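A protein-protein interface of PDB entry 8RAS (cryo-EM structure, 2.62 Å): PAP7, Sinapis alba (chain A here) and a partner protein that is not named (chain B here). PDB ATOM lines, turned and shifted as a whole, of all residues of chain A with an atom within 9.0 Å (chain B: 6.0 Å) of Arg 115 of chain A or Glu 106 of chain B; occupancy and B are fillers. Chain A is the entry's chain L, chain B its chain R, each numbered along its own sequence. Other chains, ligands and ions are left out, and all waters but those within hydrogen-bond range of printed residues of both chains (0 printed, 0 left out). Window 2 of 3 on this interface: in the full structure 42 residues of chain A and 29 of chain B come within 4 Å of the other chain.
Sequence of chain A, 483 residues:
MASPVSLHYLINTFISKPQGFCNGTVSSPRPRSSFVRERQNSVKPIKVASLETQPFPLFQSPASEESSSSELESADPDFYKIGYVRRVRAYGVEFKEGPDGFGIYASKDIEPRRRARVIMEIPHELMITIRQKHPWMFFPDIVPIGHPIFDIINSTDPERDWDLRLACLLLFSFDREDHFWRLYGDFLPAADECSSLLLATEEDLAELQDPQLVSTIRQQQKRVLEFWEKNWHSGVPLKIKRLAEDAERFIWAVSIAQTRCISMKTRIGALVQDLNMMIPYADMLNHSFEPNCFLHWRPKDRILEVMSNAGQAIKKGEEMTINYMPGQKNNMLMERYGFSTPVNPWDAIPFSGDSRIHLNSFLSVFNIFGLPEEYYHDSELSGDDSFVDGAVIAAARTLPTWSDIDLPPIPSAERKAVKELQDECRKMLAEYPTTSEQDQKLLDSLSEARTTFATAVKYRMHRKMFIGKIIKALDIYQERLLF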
ATOM      1  N   ILE A 110      13.501  11.646 -23.692  1.00  0.00           N
ATOM      2  CA  ILE A 110      14.807  11.022 -23.870  1.00  0.00           C
ATOM      3  C   ILE A 110      14.584   9.620 -24.425  1.00  0.00           C
ATOM      4  O   ILE A 110      14.065   8.739 -23.735  1.00  0.00           O
ATOM      5  CB  ILE A 110      15.600  10.994 -22.559  1.00  0.00           C
ATOM      6  CG1 ILE A 110      16.049  12.410 -22.194  1.00  0.00           C
ATOM      7  CG2 ILE A 110      16.797  10.070 -22.677  1.00  0.00           C
ATOM      8  CD1 ILE A 110      16.940  12.475 -20.985  1.00  0.00           C
ATOM      9  N   GLU A 111      14.970   9.419 -25.678  1.00  0.00           N
ATOM     10  CA  GLU A 111      14.765   8.145 -26.353  1.00  0.00           C
ATOM     11  C   GLU A 111      15.799   7.131 -25.871  1.00  0.00           C
ATOM     12  O   GLU A 111      16.999   7.415 -25.912  1.00  0.00           O
ATOM     13  CB  GLU A 111      14.866   8.332 -27.866  1.00  0.00           C
ATOM     14  CG  GLU A 111      13.986   7.404 -28.689  1.00  0.00           C
ATOM     15  CD  GLU A 111      14.442   5.962 -28.642  1.00  0.00           C
ATOM     16  OE1 GLU A 111      15.667   5.725 -28.703  1.00  0.00           O
ATOM     17  OE2 GLU A 111      13.578   5.065 -28.544  1.00  0.00           O
ATOM     18  N   PRO A 112      15.376   5.954 -25.406  1.00  0.00           N
ATOM     19  CA  PRO A 112      16.336   4.967 -24.884  1.00  0.00           C
ATOM     20  C   PRO A 112      17.229   4.429 -25.992  1.00  0.00           C
ATOM     21  O   PRO A 112      16.752   3.837 -26.962  1.00  0.00           O
ATOM     22  CB  PRO A 112      15.434   3.873 -24.301  1.00  0.00           C
ATOM     23  CG  PRO A 112      14.158   4.001 -25.061  1.00  0.00           C
ATOM     24  CD  PRO A 112      13.988   5.473 -25.318  1.00  0.00           C
ATOM     25  N   ARG A 113      18.534   4.630 -25.836  1.00  0.00           N
ATOM     26  CA  ARG A 113      19.520   4.191 -26.810  1.00  0.00           C
ATOM     27  C   ARG A 113      20.174   2.892 -26.346  1.00  0.00           C
ATOM     28  O   ARG A 113      19.845   2.337 -25.295  1.00  0.00           O
ATOM     29  CB  ARG A 113      20.563   5.286 -27.042  1.00  0.00           C
ATOM     30  CG  ARG A 113      20.006   6.543 -27.684  1.00  0.00           C
ATOM     31  CD  ARG A 113      19.341   6.230 -29.015  1.00  0.00           C
ATOM     32  NE  ARG A 113      19.749   7.156 -30.065  1.00  0.00           N
ATOM     33  CZ  ARG A 113      19.273   8.386 -30.205  1.00  0.00           C
ATOM     34  NH1 ARG A 113      18.362   8.872 -29.379  1.00  0.00           N
ATOM     35  NH2 ARG A 113      19.721   9.145 -31.200  1.00  0.00           N
ATOM     36  N   ARG A 114      21.119   2.402 -27.153  1.00  0.00           N
ATOM     37  CA  ARG A 114      21.777   1.136 -26.845  1.00  0.00           C
ATOM     38  C   ARG A 114      22.565   1.216 -25.544  1.00  0.00           C
ATOM     39  O   ARG A 114      22.522   0.289 -24.727  1.00  0.00           O
ATOM     40  CB  ARG A 114      22.691   0.728 -27.998  1.00  0.00           C
ATOM     41  CG  ARG A 114      22.099  -0.329 -28.911  1.00  0.00           C
ATOM     42  CD  ARG A 114      23.173  -1.260 -29.446  1.00  0.00           C
ATOM     43  NE  ARG A 114      24.389  -0.539 -29.802  1.00  0.00           N
ATOM     44  CZ  ARG A 114      24.715  -0.185 -31.038  1.00  0.00           C
ATOM     45  NH1 ARG A 114      23.937  -0.474 -32.068  1.00  0.00           N
ATOM     46  NH2 ARG A 114      25.850   0.476 -31.245  1.00  0.00           N
ATOM     47  N   ARG A 115      23.290   2.307 -25.334  1.00  0.00           N
ATOM     48  CA  ARG A 115      24.102   2.501 -24.144  1.00  0.00           C
ATOM     49  C   ARG A 115      23.538   3.644 -23.308  1.00  0.00           C
ATOM     50  O   ARG A 115      22.513   4.247 -23.638  1.00  0.00           O
ATOM     51  CB  ARG A 115      25.559   2.771 -24.523  1.00  0.00           C
ATOM     52  CG  ARG A 115      26.219   1.658 -25.313  1.00  0.00           C
ATOM     53  CD  ARG A 115      27.197   2.220 -26.329  1.00  0.00           C
ATOM     54  NE  ARG A 115      28.080   1.194 -26.867  1.00  0.00           N
ATOM     55  CZ  ARG A 115      28.228   0.937 -28.160  1.00  0.00           C
ATOM     56  NH1 ARG A 115      27.564   1.617 -29.080  1.00  0.00           N
ATOM     57  NH2 ARG A 115      29.064  -0.025 -28.539  1.00  0.00           N
ATOM     58  N   ALA A 116      24.222   3.932 -22.204  1.00  0.00           N
ATOM     59  CA  ALA A 116      23.837   5.049 -21.355  1.00  0.00           C
ATOM     60  C   ALA A 116      24.019   6.365 -22.100  1.00  0.00           C
ATOM     61  O   ALA A 116      24.954   6.529 -22.888  1.00  0.00           O
ATOM     62  CB  ALA A 116      24.666   5.048 -20.072  1.00  0.00           C
ATOM     63  N   ARG A 117      23.117   7.307 -21.848  1.00  0.00           N
ATOM     64  CA  ARG A 117      23.138   8.604 -22.507  1.00  0.00           C
ATOM     65  C   ARG A 117      23.704   9.660 -21.568  1.00  0.00           C
ATOM     66  O   ARG A 117      23.419   9.656 -20.367  1.00  0.00           O
ATOM     67  CB  ARG A 117      21.735   9.010 -22.958  1.00  0.00           C
ATOM     68  CG  ARG A 117      21.131   8.091 -24.001  1.00  0.00           C
ATOM     69  CD  ARG A 117      19.729   8.533 -24.370  1.00  0.00           C
ATOM     70  NE  ARG A 117      19.612   9.986 -24.407  1.00  0.00           N
ATOM     71  CZ  ARG A 117      19.303  10.686 -25.489  1.00  0.00           C
ATOM     72  NH1 ARG A 117      19.078  10.097 -26.652  1.00  0.00           N
ATOM     73  NH2 ARG A 117      19.218  12.010 -25.403  1.00  0.00           N
ATOM     74  N   VAL A 118      24.506  10.563 -22.123  1.00  0.00           N
ATOM     75  CA  VAL A 118      25.111  11.634 -21.339  1.00  0.00           C
ATOM     76  C   VAL A 118      24.050  12.689 -21.058  1.00  0.00           C
ATOM     77  O   VAL A 118      23.418  13.211 -21.981  1.00  0.00           O
ATOM     78  CB  VAL A 118      26.314  12.245 -22.070  1.00  0.00           C
ATOM     79  CG1 VAL A 118      26.922  13.365 -21.240  1.00  0.00           C
ATOM     80  CG2 VAL A 118      27.351  11.177 -22.373  1.00  0.00           C
ATOM     81  N   PHE A 294      22.906   7.826 -13.157  1.00  0.00           N
ATOM     82  CA  PHE A 294      24.034   7.472 -12.309  1.00  0.00           C
ATOM     83  C   PHE A 294      25.231   8.329 -12.691  1.00  0.00           C
ATOM     84  O   PHE A 294      25.298   8.882 -13.792  1.00  0.00           O
ATOM     85  CB  PHE A 294      24.377   5.979 -12.410  1.00  0.00           C
ATOM     86  CG  PHE A 294      24.853   5.552 -13.769  1.00  0.00           C
ATOM     87  CD1 PHE A 294      23.949   5.212 -14.758  1.00  0.00           C
ATOM     88  CD2 PHE A 294      26.207   5.474 -14.052  1.00  0.00           C
ATOM     89  CE1 PHE A 294      24.383   4.816 -16.007  1.00  0.00           C
ATOM     90  CE2 PHE A 294      26.646   5.079 -15.298  1.00  0.00           C
ATOM     91  CZ  PHE A 294      25.732   4.748 -16.276  1.00  0.00           C
ATOM     92  N   MET A 307      24.862  10.066 -16.265  1.00  0.00           N
ATOM     93  CA  MET A 307      24.431   9.184 -17.339  1.00  0.00           C
ATOM     94  C   MET A 307      23.086   8.570 -16.991  1.00  0.00           C
ATOM     95  O   MET A 307      22.918   8.008 -15.903  1.00  0.00           O
ATOM     96  CB  MET A 307      25.462   8.081 -17.591  1.00  0.00           C
ATOM     97  CG  MET A 307      26.865   8.593 -17.860  1.00  0.00           C
ATOM     98  SD  MET A 307      27.177   8.847 -19.615  1.00  0.00           S
ATOM     99  CE  MET A 307      28.410   7.587 -19.922  1.00  0.00           C
ATOM    100  N   SER A 308      22.133   8.681 -17.911  1.00  0.00           N
ATOM    101  CA  SER A 308      20.875   7.967 -17.771  1.00  0.00           C
ATOM    102  C   SER A 308      21.091   6.480 -18.025  1.00  0.00           C
ATOM    103  O   SER A 308      21.990   6.081 -18.768  1.00  0.00           O
ATOM    104  CB  SER A 308      19.832   8.522 -18.740  1.00  0.00           C
ATOM    105  OG  SER A 308      20.154   8.186 -20.076  1.00  0.00           O
ATOM    106  N   ASN A 309      20.254   5.657 -17.398  1.00  0.00           N
ATOM    107  CA  ASN A 309      20.400   4.213 -17.521  1.00  0.00           C
ATOM    108  C   ASN A 309      20.233   3.775 -18.971  1.00  0.00           C
ATOM    109  O   ASN A 309      19.414   4.323 -19.714  1.00  0.00           O
ATOM    110  CB  ASN A 309      19.382   3.500 -16.635  1.00  0.00           C
ATOM    111  CG  ASN A 309      19.686   3.652 -15.159  1.00  0.00           C
ATOM    112  OD1 ASN A 309      20.840   3.817 -14.765  1.00  0.00           O
ATOM    113  ND2 ASN A 309      18.650   3.595 -14.333  1.00  0.00           N
ATOM    114  N   ALA A 310      21.024   2.783 -19.372  1.00  0.00           N
ATOM    115  CA  ALA A 310      20.992   2.305 -20.747  1.00  0.00           C
ATOM    116  C   ALA A 310      19.682   1.585 -21.032  1.00  0.00           C
ATOM    117  O   ALA A 310      19.272   0.696 -20.279  1.00  0.00           O
ATOM    118  CB  ALA A 310      22.174   1.374 -21.011  1.00  0.00           C
ATOM    119  N   GLY A 311      19.024   1.971 -22.122  1.00  0.00           N
ATOM    120  CA  GLY A 311      17.786   1.333 -22.516  1.00  0.00           C
ATOM    121  C   GLY A 311      16.575   1.704 -21.693  1.00  0.00           C
ATOM    122  O   GLY A 311      15.532   1.058 -21.833  1.00  0.00           O
ATOM    123  N   GLN A 312      16.674   2.719 -20.839  1.00  0.00           N
ATOM    124  CA  GLN A 312      15.565   3.144 -19.991  1.00  0.00           C
ATOM    125  C   GLN A 312      14.979   4.431 -20.559  1.00  0.00           C
ATOM    126  O   GLN A 312      15.613   5.490 -20.501  1.00  0.00           O
ATOM    127  CB  GLN A 312      16.024   3.341 -18.547  1.00  0.00           C
ATOM    128  CG  GLN A 312      14.986   4.005 -17.660  1.00  0.00           C
ATOM    129  CD  GLN A 312      15.322   3.905 -16.187  1.00  0.00           C
ATOM    130  OE1 GLN A 312      16.304   3.272 -15.805  1.00  0.00           O
ATOM    131  NE2 GLN A 312      14.505   4.530 -15.351  1.00  0.00           N
ATOM    132  N   ASN B 101      39.922  -2.100 -31.853  1.00  0.00           N
ATOM    133  CA  ASN B 101      39.528  -3.498 -31.997  1.00  0.00           C
ATOM    134  C   ASN B 101      38.019  -3.667 -31.869  1.00  0.00           C
ATOM    135  O   ASN B 101      37.402  -4.408 -32.644  1.00  0.00           O
ATOM    136  CB  ASN B 101      40.254  -4.352 -30.958  1.00  0.00           C
ATOM    137  CG  ASN B 101      41.636  -4.766 -31.411  1.00  0.00           C
ATOM    138  OD1 ASN B 101      41.908  -4.853 -32.606  1.00  0.00           O
ATOM    139  ND2 ASN B 101      42.519  -5.022 -30.455  1.00  0.00           N
ATOM    140  N   SER B 102      37.406  -2.988 -30.896  1.00  0.00           N
ATOM    141  CA  SER B 102      35.961  -3.093 -30.716  1.00  0.00           C
ATOM    142  C   SER B 102      35.208  -2.493 -31.895  1.00  0.00           C
ATOM    143  O   SER B 102      34.192  -3.045 -32.336  1.00  0.00           O
ATOM    144  CB  SER B 102      35.547  -2.417 -29.411  1.00  0.00           C
ATOM    145  OG  SER B 102      35.856  -1.037 -29.436  1.00  0.00           O
ATOM    146  N   VAL B 103      35.690  -1.364 -32.422  1.00  0.00           N
ATOM    147  CA  VAL B 103      35.054  -0.762 -33.590  1.00  0.00           C
ATOM    148  C   VAL B 103      35.141  -1.702 -34.785  1.00  0.00           C
ATOM    149  O   VAL B 103      34.167  -1.878 -35.528  1.00  0.00           O
ATOM    150  CB  VAL B 103      35.687   0.609 -33.894  1.00  0.00           C
ATOM    151  CG1 VAL B 103      35.350   1.055 -35.306  1.00  0.00           C
ATOM    152  CG2 VAL B 103      35.220   1.642 -32.886  1.00  0.00           C
ATOM    153  N   ALA B 104      36.303  -2.326 -34.984  1.00  0.00           N
ATOM    154  CA  ALA B 104      36.459  -3.263 -36.092  1.00  0.00           C
ATOM    155  C   ALA B 104      35.544  -4.470 -35.930  1.00  0.00           C
ATOM    156  O   ALA B 104      34.952  -4.941 -36.906  1.00  0.00           O
ATOM    157  CB  ALA B 104      37.917  -3.703 -36.207  1.00  0.00           C
ATOM    158  N   ALA B 105      35.417  -4.986 -34.705  1.00  0.00           N
ATOM    159  CA  ALA B 105      34.531  -6.124 -34.472  1.00  0.00           C
ATOM    160  C   ALA B 105      33.076  -5.759 -34.741  1.00  0.00           C
ATOM    161  O   ALA B 105      32.331  -6.540 -35.349  1.00  0.00           O
ATOM    162  CB  ALA B 105      34.701  -6.638 -33.044  1.00  0.00           C
ATOM    163  N   GLU B 106      32.649  -4.575 -34.294  1.00  0.00           N
ATOM    164  CA  GLU B 106      31.277  -4.145 -34.543  1.00  0.00           C
ATOM    165  C   GLU B 106      31.018  -3.955 -36.032  1.00  0.00           C
ATOM    166  O   GLU B 106      29.953  -4.329 -36.539  1.00  0.00           O
ATOM    167  CB  GLU B 106      30.986  -2.859 -33.773  1.00  0.00           C
ATOM    168  CG  GLU B 106      29.509  -2.576 -33.582  1.00  0.00           C
ATOM    169  CD  GLU B 106      29.259  -1.331 -32.760  1.00  0.00           C
ATOM    170  OE1 GLU B 106      30.161  -0.935 -31.994  1.00  0.00           O
ATOM    171  OE2 GLU B 106      28.163  -0.747 -32.879  1.00  0.00           O
ATOM    172  N   ALA B 107      31.982  -3.376 -36.754  1.00  0.00           N
ATOM    173  CA  ALA B 107      31.834  -3.222 -38.197  1.00  0.00           C
ATOM    174  C   ALA B 107      31.766  -4.577 -38.891  1.00  0.00           C
ATOM    175  O   ALA B 107      31.000  -4.758 -39.846  1.00  0.00           O
ATOM    176  CB  ALA B 107      32.983  -2.388 -38.758  1.00  0.00           C
ATOM    177  N   THR B 108      32.570  -5.539 -38.431  1.00  0.00           N
ATOM    178  CA  THR B 108      32.515  -6.882 -38.996  1.00  0.00           C
ATOM    179  C   THR B 108      31.145  -7.510 -38.780  1.00  0.00           C
ATOM    180  O   THR B 108      30.588  -8.129 -39.693  1.00  0.00           O
ATOM    181  CB  THR B 108      33.611  -7.752 -38.382  1.00  0.00           C
ATOM    182  OG1 THR B 108      34.894  -7.254 -38.774  1.00  0.00           O
ATOM    183  CG2 THR B 108      33.474  -9.192 -38.844  1.00  0.00           C
ATOM    184  N   GLU B 109      30.585  -7.356 -37.578  1.00  0.00           N
ATOM    185  CA  GLU B 109      29.240  -7.868 -37.324  1.00  0.00           C
ATOM    186  C   GLU B 109      28.217  -7.197 -38.233  1.00  0.00           C
ATOM    187  O   GLU B 109      27.321  -7.862 -38.769  1.00  0.00           O
ATOM    188  CB  GLU B 109      28.864  -7.666 -35.858  1.00  0.00           C
ATOM    189  CG  GLU B 109      29.702  -8.469 -34.884  1.00  0.00           C
ATOM    190  CD  GLU B 109      29.511  -8.015 -33.452  1.00  0.00           C
ATOM    191  OE1 GLU B 109      28.697  -7.095 -33.222  1.00  0.00           O
ATOM    192  OE2 GLU B 109      30.175  -8.577 -32.555  1.00  0.00           O
ATOM    193  N   TYR B 110      28.333  -5.877 -38.413  1.00  0.00           N
ATOM    194  CA  TYR B 110      27.432  -5.166 -39.316  1.00  0.00           C
ATOM    195  C   TYR B 110      27.506  -5.733 -40.726  1.00  0.00           C
ATOM    196  O   TYR B 110      26.476  -5.940 -41.376  1.00  0.00           O
ATOM    197  CB  TYR B 110      27.770  -3.675 -39.343  1.00  0.00           C
ATOM    198  CG  TYR B 110      27.298  -2.879 -38.150  1.00  0.00           C
ATOM    199  CD1 TYR B 110      26.798  -3.504 -37.018  1.00  0.00           C
ATOM    200  CD2 TYR B 110      27.351  -1.492 -38.162  1.00  0.00           C
ATOM    201  CE1 TYR B 110      26.369  -2.770 -35.930  1.00  0.00           C
ATOM    202  CE2 TYR B 110      26.924  -0.752 -37.083  1.00  0.00           C
ATOM    203  CZ  TYR B 110      26.435  -1.394 -35.970  1.00  0.00           C
ATOM    204  OH  TYR B 110      26.008  -0.655 -34.891  1.00  0.00           O
ATOM    205  N   VAL B 111      28.721  -5.982 -41.218  1.00  0.00           N
ATOM    206  CA  VAL B 111      28.879  -6.477 -42.583  1.00  0.00           C
ATOM    207  C   VAL B 111      28.325  -7.890 -42.713  1.00  0.00           C
ATOM    208  O   VAL B 111      27.658  -8.217 -43.701  1.00  0.00           O
ATOM    209  CB  VAL B 111      30.354  -6.401 -43.013  1.00  0.00           C
ATOM    210  CG1 VAL B 111      30.564  -7.141 -44.321  1.00  0.00           C
ATOM    211  CG2 VAL B 111      30.777  -4.960 -43.160  1.00  0.00           C
ATOM    212  N   VAL B 128      29.356   2.400 -37.673  1.00  0.00           N
ATOM    213  CA  VAL B 128      29.665   2.079 -36.282  1.00  0.00           C
ATOM    214  C   VAL B 128      29.967   3.350 -35.501  1.00  0.00           C
ATOM    215  O   VAL B 128      29.481   3.543 -34.380  1.00  0.00           O
ATOM    216  CB  VAL B 128      30.835   1.082 -36.210  1.00  0.00           C
ATOM    217  CG1 VAL B 128      31.399   1.016 -34.805  1.00  0.00           C
ATOM    218  CG2 VAL B 128      30.386  -0.289 -36.665  1.00  0.00           C
ATOM    219  N   ASN B 131      26.757   5.353 -34.966  1.00  0.00           N
ATOM    220  CA  ASN B 131      25.910   4.716 -33.964  1.00  0.00           C
ATOM    221  C   ASN B 131      26.461   4.923 -32.560  1.00  0.00           C
ATOM    222  O   ASN B 131      25.700   5.171 -31.619  1.00  0.00           O
ATOM    223  CB  ASN B 131      25.767   3.227 -34.269  1.00  0.00           C
ATOM    224  CG  ASN B 131      24.668   2.943 -35.265  1.00  0.00           C
ATOM    225  OD1 ASN B 131      23.960   3.850 -35.700  1.00  0.00           O
ATOM    226  ND2 ASN B 131      24.519   1.679 -35.636  1.00  0.00           N
ATOM    227  N   ARG B 132      27.780   4.817 -32.397  1.00  0.00           N
ATOM    228  CA  ARG B 132      28.379   5.050 -31.087  1.00  0.00           C
ATOM    229  C   ARG B 132      28.196   6.496 -30.649  1.00  0.00           C
ATOM    230  O   ARG B 132      27.985   6.768 -29.462  1.00  0.00           O
ATOM    231  CB  ARG B 132      29.858   4.671 -31.109  1.00  0.00           C
ATOM    232  CG  ARG B 132      30.094   3.185 -31.288  1.00  0.00           C
ATOM    233  CD  ARG B 132      31.403   2.737 -30.676  1.00  0.00           C
ATOM    234  NE  ARG B 132      31.654   1.326 -30.940  1.00  0.00           N
ATOM    235  CZ  ARG B 132      32.562   0.595 -30.312  1.00  0.00           C
ATOM    236  NH1 ARG B 132      33.333   1.111 -29.370  1.00  0.00           N
ATOM    237  NH2 ARG B 132      32.699  -0.687 -30.635  1.00  0.00           N
ATOM    238  N   ASP B 135      24.500   6.792 -29.798  1.00  0.00           N
ATOM    239  CA  ASP B 135      24.170   6.137 -28.536  1.00  0.00           C
ATOM    240  C   ASP B 135      24.328   7.067 -27.342  1.00  0.00           C
ATOM    241  O   ASP B 135      23.684   6.848 -26.311  1.00  0.00           O
ATOM    242  CB  ASP B 135      25.039   4.896 -28.343  1.00  0.00           C
ATOM    243  CG  ASP B 135      24.544   3.710 -29.141  1.00  0.00           C
ATOM    244  OD1 ASP B 135      25.265   2.692 -29.203  1.00  0.00           O
ATOM    245  OD2 ASP B 135      23.434   3.795 -29.707  1.00  0.00           O
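Of the 15 printed residues of chain B, 4 touch a printed residue of chain A.
Hydrophobic or aromatic side chains of chain B within 4 Å of the printed part of chain A: Tyr 110.
Along chain B the printed residues that touch a printed residue of chain A span positions 106 to 135.
Of the 16 printed residues of chain A, 5 touch a printed residue of chain B.
Among the printed residues, merely in contact across the chains: Arg 113 of chain A with Asp 135 of chain B (3.6 Å), Arg 114 of chain A with Tyr 110 of chain B (3.5 Å), Arg 115 of chain A with Arg 132 of chain B (3.7 Å), Ala 116 of chain A with Asp 135 of chain B (3.7 Å) and Arg 117 of chain A with Asp 135 of chain B (3.7 Å).
The guanidinium group (NH2) of Arg 114 of chain A is in salt-bridge range of the side-chain carboxylate (OE2) of Glu 106 of chain B, at 3.1 Å.
The side-chain carboxylate of Glu 106 of chain B lies within salt-bridge range of the guanidinium group of Arg 115 of chain A, at 3.7 Å.
The guanidinium group (NH1) of Arg 115 of chain A is in salt-bridge range of the side-chain carboxylate (OD1) of Asp 135 of chain B (2.5 Å).
The guanidinium group (NH2) of Arg 114 of chain A lies within salt-bridge range of the side-chain carboxylate (OD1) of Asp 135 of chain B (3.1 Å).
Of the printed residues of chain B, Arg 114 of chain A touches Glu 106, Tyr 110 and Asp 135.
Of chain B, only Glu 106, Arg 132 and Asp 135 come within 4 Å of Arg 115 of chain A.
Printed residues of chain B within 4 Å of Arg 117 of chain A: Asp 135.
Ser 308 of chain A touches none of the printed residues of chain B.
No residue of chain A comes within 4 Å of Ala 105 of chain B.
Glu 106 of chain B touches just these residues of chain A: Arg 114 (3.1 Å) and Arg 115 (3.7 Å).
Of the printed residues of chain A, Arg 132 of chain B touches Arg 115.
Of the printed residues of chain A, Asp 135 of chain B touches Arg 113 (3.6 Å), Arg 114 (3.1 Å), Arg 115 (2.5 Å), Ala 116 (3.7 Å) and Arg 117 (3.7 Å).
The nearest residue of chain B that does not touch Arg 115 of chain A is Asn 131 of chain B (4.7 Å).
The nearest printed residue of chain B that does not touch Arg 114 of chain A is Asn 131 of chain B (4.1 Å).
The side-chain carboxylate of Glu 106 of chain B is in salt-bridge range of the guanidinium group of Arg 132 of chain B, 2.9 Å away.
O of Ser 102 of chain B is in hydrogen-bond range of NH2 of Arg 132 of chain B, 3.3 Å away.
The backbone carbonyl oxygen (O) of Arg 113 of chain A lies within hydrogen-bond range of the backbone NH (N) of Gly 311 of chain A (3.3 Å).
The backbone carbonyl oxygen (O) of Arg 117 of chain A lies within hydrogen-bond range of the backbone NH (N) of Ser 308 of chain A.
The backbone carbonyl oxygen (O) of Glu 111 of chain A lies close to the guanidinium group (NH1) of Arg 117 of chain A (3.5 Å).
The side-chain hydroxyl (OH) of Tyr 110 of chain B is in hydrogen-bond range of the side-chain amide nitrogen (ND2) of Asn 131 of chain B.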
